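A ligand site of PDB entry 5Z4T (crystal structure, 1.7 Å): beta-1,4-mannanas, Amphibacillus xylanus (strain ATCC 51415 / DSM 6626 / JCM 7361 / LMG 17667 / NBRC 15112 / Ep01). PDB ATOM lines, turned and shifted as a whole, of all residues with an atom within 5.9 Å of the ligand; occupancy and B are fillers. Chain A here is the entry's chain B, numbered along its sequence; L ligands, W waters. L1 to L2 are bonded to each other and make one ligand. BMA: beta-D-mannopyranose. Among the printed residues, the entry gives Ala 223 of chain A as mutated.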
ATOM      1  N   TRP A  11     -23.564  -6.903   2.992  1.00  0.00           N
ATOM      2  CA  TRP A  11     -23.669  -7.052   1.541  1.00  0.00           C
ATOM      3  C   TRP A  11     -22.746  -8.153   1.015  1.00  0.00           C
ATOM      4  O   TRP A  11     -23.108  -8.860   0.065  1.00  0.00           O
ATOM      5  CB  TRP A  11     -23.348  -5.722   0.845  1.00  0.00           C
ATOM      6  CG  TRP A  11     -23.591  -5.722  -0.653  1.00  0.00           C
ATOM      7  CD1 TRP A  11     -22.675  -5.469  -1.631  1.00  0.00           C
ATOM      8  CD2 TRP A  11     -24.840  -5.941  -1.314  1.00  0.00           C
ATOM      9  NE1 TRP A  11     -23.277  -5.517  -2.863  1.00  0.00           N
ATOM     10  CE2 TRP A  11     -24.601  -5.808  -2.697  1.00  0.00           C
ATOM     11  CE3 TRP A  11     -26.135  -6.234  -0.871  1.00  0.00           C
ATOM     12  CZ2 TRP A  11     -25.622  -5.947  -3.652  1.00  0.00           C
ATOM     13  CZ3 TRP A  11     -27.150  -6.375  -1.818  1.00  0.00           C
ATOM     14  CH2 TRP A  11     -26.883  -6.237  -3.192  1.00  0.00           C
ATOM     15  N   LYS A  85     -33.358  -5.528   4.113  1.00  0.00           N
ATOM     16  CA  LYS A  85     -33.349  -5.120   2.711  1.00  0.00           C
ATOM     17  C   LYS A  85     -32.992  -6.316   1.839  1.00  0.00           C
ATOM     18  O   LYS A  85     -31.826  -6.487   1.449  1.00  0.00           O
ATOM     19  CB  LYS A  85     -32.374  -3.945   2.504  1.00  0.00           C
ATOM     20  CG  LYS A  85     -32.239  -3.436   1.066  1.00  0.00           C
ATOM     21  CD  LYS A  85     -31.445  -2.118   1.036  1.00  0.00           C
ATOM     22  CE  LYS A  85     -30.823  -1.857  -0.329  1.00  0.00           C
ATOM     23  NZ  LYS A  85     -30.125  -0.531  -0.380  1.00  0.00           N
ATOM     24  N   ASN A  89     -29.633 -10.186  -7.200  1.00  0.00           N
ATOM     25  CA  ASN A  89     -28.605  -9.974  -8.214  1.00  0.00           C
ATOM     26  C   ASN A  89     -28.742 -11.041  -9.293  1.00  0.00           C
ATOM     27  O   ASN A  89     -29.417 -12.058  -9.117  1.00  0.00           O
ATOM     28  CB  ASN A  89     -27.198 -10.023  -7.595  1.00  0.00           C
ATOM     29  CG  ASN A  89     -26.933  -8.841  -6.685  1.00  0.00           C
ATOM     30  OD1 ASN A  89     -27.551  -7.789  -6.805  1.00  0.00           O
ATOM     31  ND2 ASN A  89     -26.029  -9.021  -5.735  1.00  0.00           N
ATOM     32  N   TRP A  95     -26.833  -5.752 -13.785  1.00  0.00           N
ATOM     33  CA  TRP A  95     -27.439  -4.991 -12.699  1.00  0.00           C
ATOM     34  C   TRP A  95     -28.950  -5.199 -12.669  1.00  0.00           C
ATOM     35  O   TRP A  95     -29.598  -5.257 -13.714  1.00  0.00           O
ATOM     36  CB  TRP A  95     -27.094  -3.507 -12.890  1.00  0.00           C
ATOM     37  CG  TRP A  95     -27.655  -2.516 -11.893  1.00  0.00           C
ATOM     38  CD1 TRP A  95     -27.955  -2.713 -10.566  1.00  0.00           C
ATOM     39  CD2 TRP A  95     -27.948  -1.143 -12.178  1.00  0.00           C
ATOM     40  NE1 TRP A  95     -28.426  -1.534 -10.009  1.00  0.00           N
ATOM     41  CE2 TRP A  95     -28.426  -0.562 -10.974  1.00  0.00           C
ATOM     42  CE3 TRP A  95     -27.860  -0.334 -13.327  1.00  0.00           C
ATOM     43  CZ2 TRP A  95     -28.824   0.785 -10.903  1.00  0.00           C
ATOM     44  CZ3 TRP A  95     -28.241   0.989 -13.251  1.00  0.00           C
ATOM     45  CH2 TRP A  95     -28.720   1.545 -12.042  1.00  0.00           C
ATOM     46  N   ARG A  96     -29.507  -5.334 -11.464  1.00  0.00           N
ATOM     47  CA  ARG A  96     -30.918  -5.676 -11.320  1.00  0.00           C
ATOM     48  C   ARG A  96     -31.854  -4.624 -11.913  1.00  0.00           C
ATOM     49  O   ARG A  96     -33.019  -4.930 -12.176  1.00  0.00           O
ATOM     50  CB  ARG A  96     -31.257  -5.921  -9.848  1.00  0.00           C
ATOM     51  CG  ARG A  96     -31.265  -4.653  -8.993  1.00  0.00           C
ATOM     52  CD  ARG A  96     -31.278  -5.004  -7.494  1.00  0.00           C
ATOM     53  NE  ARG A  96     -29.957  -5.403  -7.009  1.00  0.00           N
ATOM     54  CZ  ARG A  96     -28.965  -4.555  -6.741  1.00  0.00           C
ATOM     55  NH1 ARG A  96     -29.152  -3.257  -6.909  1.00  0.00           N
ATOM     56  NH2 ARG A  96     -27.797  -5.003  -6.334  1.00  0.00           N
ATOM     57  N   CYS A 142     -35.040  -2.793  -4.621  1.00  0.00           N
ATOM     58  CA  CYS A 142     -33.855  -1.944  -4.674  1.00  0.00           C
ATOM     59  C   CYS A 142     -33.488  -1.705  -6.129  1.00  0.00           C
ATOM     60  O   CYS A 142     -33.107  -2.636  -6.830  1.00  0.00           O
ATOM     61  CB  CYS A 142     -32.689  -2.600  -3.927  1.00  0.00           C
ATOM     62  SG  CYS A 142     -31.148  -1.685  -4.003  1.00  0.00           S
ATOM     63  N   GLU A 143     -33.612  -0.453  -6.588  1.00  0.00           N
ATOM     64  CA  GLU A 143     -33.094  -0.012  -7.889  1.00  0.00           C
ATOM     65  C   GLU A 143     -33.671  -0.819  -9.054  1.00  0.00           C
ATOM     66  O   GLU A 143     -32.972  -1.051 -10.051  1.00  0.00           O
ATOM     67  CB  GLU A 143     -31.560  -0.050  -7.916  1.00  0.00           C
ATOM     68  CG  GLU A 143     -30.893   0.847  -6.866  1.00  0.00           C
ATOM     69  CD  GLU A 143     -29.397   0.573  -6.650  1.00  0.00           C
ATOM     70  OE1 GLU A 143     -28.770   1.317  -5.859  1.00  0.00           O
ATOM     71  OE2 GLU A 143     -28.843  -0.385  -7.250  1.00  0.00           O
ATOM     72  N   ASN A 172     -36.825   1.146  -2.418  1.00  0.00           N
ATOM     73  CA  ASN A 172     -35.599   1.886  -2.706  1.00  0.00           C
ATOM     74  C   ASN A 172     -35.381   2.106  -4.195  1.00  0.00           C
ATOM     75  O   ASN A 172     -34.959   1.182  -4.895  1.00  0.00           O
ATOM     76  CB  ASN A 172     -34.445   1.089  -2.096  1.00  0.00           C
ATOM     77  CG  ASN A 172     -33.072   1.662  -2.399  1.00  0.00           C
ATOM     78  OD1 ASN A 172     -32.060   1.059  -2.041  1.00  0.00           O
ATOM     79  ND2 ASN A 172     -33.012   2.819  -3.045  1.00  0.00           N
ATOM     80  N   SER A 193     -31.427   5.554  -3.675  1.00  0.00           N
ATOM     81  CA  SER A 193     -29.968   5.473  -3.618  1.00  0.00           C
ATOM     82  C   SER A 193     -29.421   6.842  -4.027  1.00  0.00           C
ATOM     83  O   SER A 193     -29.313   7.147  -5.207  1.00  0.00           O
ATOM     84  CB  SER A 193     -29.448   4.382  -4.560  1.00  0.00           C
ATOM     85  OG  SER A 193     -29.934   3.103  -4.174  1.00  0.00           O
ATOM     86  N   TYR A 195     -26.887   8.633  -4.802  1.00  0.00           N
ATOM     87  CA  TYR A 195     -25.512   8.687  -5.314  1.00  0.00           C
ATOM     88  C   TYR A 195     -25.354   9.902  -6.227  1.00  0.00           C
ATOM     89  O   TYR A 195     -25.206   9.802  -7.442  1.00  0.00           O
ATOM     90  CB  TYR A 195     -25.177   7.403  -6.053  1.00  0.00           C
ATOM     91  CG  TYR A 195     -24.985   6.166  -5.188  1.00  0.00           C
ATOM     92  CD1 TYR A 195     -24.036   6.155  -4.162  1.00  0.00           C
ATOM     93  CD2 TYR A 195     -25.707   5.016  -5.421  1.00  0.00           C
ATOM     94  CE1 TYR A 195     -23.843   5.019  -3.376  1.00  0.00           C
ATOM     95  CE2 TYR A 195     -25.520   3.855  -4.653  1.00  0.00           C
ATOM     96  CZ  TYR A 195     -24.570   3.871  -3.618  1.00  0.00           C
ATOM     97  OH  TYR A 195     -24.377   2.746  -2.841  1.00  0.00           O
ATOM     98  N   ALA A 223     -29.609   4.240   0.635  1.00  0.00           N
ATOM     99  CA  ALA A 223     -28.221   4.005   0.279  1.00  0.00           C
ATOM    100  C   ALA A 223     -27.577   5.326  -0.122  1.00  0.00           C
ATOM    101  O   ALA A 223     -28.214   6.151  -0.773  1.00  0.00           O
ATOM    102  CB  ALA A 223     -28.087   2.990  -0.846  1.00  0.00           C
ATOM    103  N   PRO A 236     -20.389   8.520  -7.665  1.00  0.00           N
ATOM    104  CA  PRO A 236     -20.152   7.713  -6.454  1.00  0.00           C
ATOM    105  C   PRO A 236     -20.827   6.342  -6.494  1.00  0.00           C
ATOM    106  O   PRO A 236     -20.438   5.477  -5.696  1.00  0.00           O
ATOM    107  CB  PRO A 236     -20.712   8.585  -5.323  1.00  0.00           C
ATOM    108  CG  PRO A 236     -21.704   9.490  -5.990  1.00  0.00           C
ATOM    109  CD  PRO A 236     -21.139   9.755  -7.367  1.00  0.00           C
ATOM    110  N   ASN A 237     -21.808   6.137  -7.360  1.00  0.00           N
ATOM    111  CA  ASN A 237     -22.452   4.837  -7.521  1.00  0.00           C
ATOM    112  C   ASN A 237     -21.561   3.843  -8.238  1.00  0.00           C
ATOM    113  O   ASN A 237     -21.866   2.641  -8.227  1.00  0.00           O
ATOM    114  CB  ASN A 237     -23.723   4.989  -8.342  1.00  0.00           C
ATOM    115  CG  ASN A 237     -23.434   5.595  -9.713  1.00  0.00           C
ATOM    116  OD1 ASN A 237     -23.045   6.755  -9.804  1.00  0.00           O
ATOM    117  ND2 ASN A 237     -23.555   4.787 -10.765  1.00  0.00           N
ATOM    118  N   LYS A 238     -20.504   4.305  -8.905  1.00  0.00           N
ATOM    119  CA  LYS A 238     -19.781   3.453  -9.850  1.00  0.00           C
ATOM    120  C   LYS A 238     -18.752   2.637  -9.091  1.00  0.00           C
ATOM    121  O   LYS A 238     -17.603   3.028  -8.927  1.00  0.00           O
ATOM    122  CB  LYS A 238     -19.112   4.298 -10.930  1.00  0.00           C
ATOM    123  CG  LYS A 238     -20.004   4.580 -12.126  1.00  0.00           C
ATOM    124  CD  LYS A 238     -19.219   4.496 -13.439  1.00  0.00           C
ATOM    125  CE  LYS A 238     -20.118   4.771 -14.633  1.00  0.00           C
ATOM    126  NZ  LYS A 238     -21.106   3.689 -14.845  1.00  0.00           N
ATOM    127  N   TRP A 239     -19.182   1.453  -8.635  1.00  0.00           N
ATOM    128  CA  TRP A 239     -18.319   0.620  -7.824  1.00  0.00           C
ATOM    129  C   TRP A 239     -17.113   0.110  -8.611  1.00  0.00           C
ATOM    130  O   TRP A 239     -16.093  -0.230  -8.010  1.00  0.00           O
ATOM    131  CB  TRP A 239     -19.104  -0.548  -7.232  1.00  0.00           C
ATOM    132  CG  TRP A 239     -19.973  -1.295  -8.239  1.00  0.00           C
ATOM    133  CD1 TRP A 239     -21.283  -1.029  -8.565  1.00  0.00           C
ATOM    134  CD2 TRP A 239     -19.584  -2.412  -9.031  1.00  0.00           C
ATOM    135  NE1 TRP A 239     -21.725  -1.927  -9.501  1.00  0.00           N
ATOM    136  CE2 TRP A 239     -20.702  -2.789  -9.804  1.00  0.00           C
ATOM    137  CE3 TRP A 239     -18.408  -3.168  -9.138  1.00  0.00           C
ATOM    138  CZ2 TRP A 239     -20.671  -3.863 -10.684  1.00  0.00           C
ATOM    139  CZ3 TRP A 239     -18.376  -4.231 -10.027  1.00  0.00           C
ATOM    140  CH2 TRP A 239     -19.500  -4.575 -10.786  1.00  0.00           C
ATOM    141  N   TRP A 273     -23.392   3.288   2.507  1.00  0.00           N
ATOM    142  CA  TRP A 273     -22.917   2.116   1.789  1.00  0.00           C
ATOM    143  C   TRP A 273     -21.393   2.124   1.758  1.00  0.00           C
ATOM    144  O   TRP A 273     -20.805   3.053   1.191  1.00  0.00           O
ATOM    145  CB  TRP A 273     -23.465   2.120   0.353  1.00  0.00           C
ATOM    146  CG  TRP A 273     -23.292   0.798  -0.293  1.00  0.00           C
ATOM    147  CD1 TRP A 273     -22.141   0.296  -0.830  1.00  0.00           C
ATOM    148  CD2 TRP A 273     -24.284  -0.202  -0.413  1.00  0.00           C
ATOM    149  NE1 TRP A 273     -22.378  -0.987  -1.298  1.00  0.00           N
ATOM    150  CE2 TRP A 273     -23.684  -1.303  -1.052  1.00  0.00           C
ATOM    151  CE3 TRP A 273     -25.621  -0.273  -0.055  1.00  0.00           C
ATOM    152  CZ2 TRP A 273     -24.387  -2.476  -1.330  1.00  0.00           C
ATOM    153  CZ3 TRP A 273     -26.329  -1.443  -0.341  1.00  0.00           C
ATOM    154  CH2 TRP A 273     -25.706  -2.523  -0.976  1.00  0.00           C
ATOM    155  N   TYR A 291     -15.792   1.371  -0.760  1.00  0.00           N
ATOM    156  CA  TYR A 291     -16.771   2.212  -0.074  1.00  0.00           C
ATOM    157  C   TYR A 291     -16.538   2.297   1.434  1.00  0.00           C
ATOM    158  O   TYR A 291     -17.002   3.256   2.074  1.00  0.00           O
ATOM    159  CB  TYR A 291     -18.198   1.693  -0.299  1.00  0.00           C
ATOM    160  CG  TYR A 291     -18.754   1.978  -1.686  1.00  0.00           C
ATOM    161  CD1 TYR A 291     -19.454   3.147  -1.936  1.00  0.00           C
ATOM    162  CD2 TYR A 291     -18.595   1.073  -2.717  1.00  0.00           C
ATOM    163  CE1 TYR A 291     -19.972   3.412  -3.194  1.00  0.00           C
ATOM    164  CE2 TYR A 291     -19.114   1.314  -3.970  1.00  0.00           C
ATOM    165  CZ  TYR A 291     -19.797   2.499  -4.200  1.00  0.00           C
ATOM    166  OH  TYR A 291     -20.316   2.778  -5.454  1.00  0.00           O
HETATM  167  C1  BMA L   1     -26.058  -0.180  -4.102  1.00  0.00           C
HETATM  168  C2  BMA L   1     -26.322  -1.301  -5.104  1.00  0.00           C
HETATM  169  C3  BMA L   1     -25.199  -2.273  -5.074  1.00  0.00           C
HETATM  170  C4  BMA L   1     -23.857  -1.639  -5.312  1.00  0.00           C
HETATM  171  C5  BMA L   1     -23.639  -0.432  -4.389  1.00  0.00           C
HETATM  172  C6  BMA L   1     -22.376   0.326  -4.708  1.00  0.00           C
HETATM  173  O1  BMA L   1     -27.070   0.756  -4.067  1.00  0.00           O
HETATM  174  O2  BMA L   1     -26.379  -0.754  -6.431  1.00  0.00           O
HETATM  175  O3  BMA L   1     -25.484  -3.290  -6.078  1.00  0.00           O
HETATM  176  O4  BMA L   1     -22.732  -2.487  -4.910  1.00  0.00           O
HETATM  177  O5  BMA L   1     -24.783   0.497  -4.468  1.00  0.00           O
HETATM  178  O6  BMA L   1     -22.493   0.862  -5.999  1.00  0.00           O
HETATM  179  C1  BMA L   2     -22.223  -3.316  -5.858  1.00  0.00           C
HETATM  180  C2  BMA L   2     -20.803  -3.749  -5.497  1.00  0.00           C
HETATM  181  C3  BMA L   2     -20.236  -4.653  -6.556  1.00  0.00           C
HETATM  182  C4  BMA L   2     -21.075  -5.630  -6.818  1.00  0.00           C
HETATM  183  C5  BMA L   2     -22.740  -5.365  -7.026  1.00  0.00           C
HETATM  184  C6  BMA L   2     -23.566  -6.597  -7.009  1.00  0.00           C
HETATM  185  O2  BMA L   2     -20.769  -4.344  -4.183  1.00  0.00           O
HETATM  186  O3  BMA L   2     -19.023  -5.347  -6.123  1.00  0.00           O
HETATM  187  O4  BMA L   2     -21.030  -6.863  -7.981  1.00  0.00           O
HETATM  188  O5  BMA L   2     -23.082  -4.529  -5.875  1.00  0.00           O
HETATM  189  O6  BMA L   2     -24.867  -6.208  -7.079  1.00  0.00           O
HETATM  190  O   HOH W   1     -24.917   1.525  -7.464  1.00  0.00           O
HETATM  191  O   HOH W   2     -21.040  -9.410  -6.751  1.00  0.00           O
HETATM  192  O   HOH W   3     -25.192  -2.095  -8.701  1.00  0.00           O
HETATM  193  O   HOH W   4     -16.876  -3.468  -5.557  1.00  0.00           O
HETATM  194  O   HOH W   5     -20.147  -2.642  -2.320  1.00  0.00           O
HETATM  195  O   HOH W   6     -18.498  -5.958  -3.403  1.00  0.00           O
HETATM  196  O   HOH W   7     -29.136   0.498  -2.545  1.00  0.00           O
HETATM  197  O   HOH W   8     -25.316  -4.795  -9.522  1.00  0.00           O
HETATM  198  O   HOH W   9     -17.572  -7.153  -7.680  1.00  0.00           O
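Water W7 lies within hydrogen-bond range of O1 of BMA L1 (2.6 Å), NZ of Lys 85 (2.6 Å), OD1 of Asn 172 (3.0 Å), OG of Ser 193 (3.2 Å), SG of Cys 142 (3.3 Å) and OE1 of Glu 143 (3.4 Å). Water W5 lies within hydrogen-bond range of O2 of BMA L2 and NE1 of Trp 273. Water W1 bridges an oxygen (O2) of BMA L1 and the backbone carbonyl oxygen (O) of Asn 237.
The side-chain carboxylate (OE2) of Glu 143 is in salt-bridge range of the guanidinium group (NH1) of Arg 96. OE1 of Glu 143 sits at hydrogen-bond distance from OG of Ser 193 (2.7 Å). OE2 of Glu 143 is in hydrogen-bond range of NE1 of Trp 95 (3.0 Å). The backbone NH of Glu 143 lies within hydrogen-bond range of the backbone carbonyl oxygen of Asn 172. The guanidinium group (NH2) of Arg 96 lies within hydrogen-bond range of the side-chain amide oxygen (OD1) of Asn 89 (2.8 Å). The backbone carbonyl oxygen (O) of Asn 237 is in hydrogen-bond range of the side-chain hydroxyl (OH) of Tyr 291 (3.2 Å). The backbone carbonyl oxygen (O) of Pro 236 lies within hydrogen-bond range of the side-chain hydroxyl (OH) of Tyr 291 (2.7 Å). The side-chain amide nitrogen of Asn 172 sits close to the backbone NH of Ser 193.
O1 of BMA L1 sits at hydrogen-bond distance from OE1 of Glu 143 (2.5 Å). The side-chain hydroxyl (OH) of Tyr 195 is in hydrogen-bond range of an oxygen (O5) of BMA L1 (2.8 Å). O3 of BMA L1 sits at hydrogen-bond distance from NH2 of Arg 96 (2.9 Å). O of Asn 237 is in hydrogen-bond range of O6 of BMA L1, 2.9 Å away. OH of Tyr 291 lies within hydrogen-bond range of O6 of BMA L1 (3.0 Å). The indole nitrogen (NE1) of Trp 11 is in hydrogen-bond range of an oxygen (O2) of BMA L2 (3.1 Å). The side-chain amide oxygen (OD1) of Asn 89 lies within hydrogen-bond range of an oxygen (O6) of BMA L2 (3.1 Å).
Merely in contact with the ligand: Ser 193 (3.7 Å), Trp 239 (3.4 Å) and Trp 273 (3.4 Å). Hydrophobic or aromatic side chains that line the ligand: Trp 11, Tyr 195, Trp 239, Trp 273 and Tyr 291. The nearest printed residue that does not touch the ligand is Ala 223 (4.05 Å).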
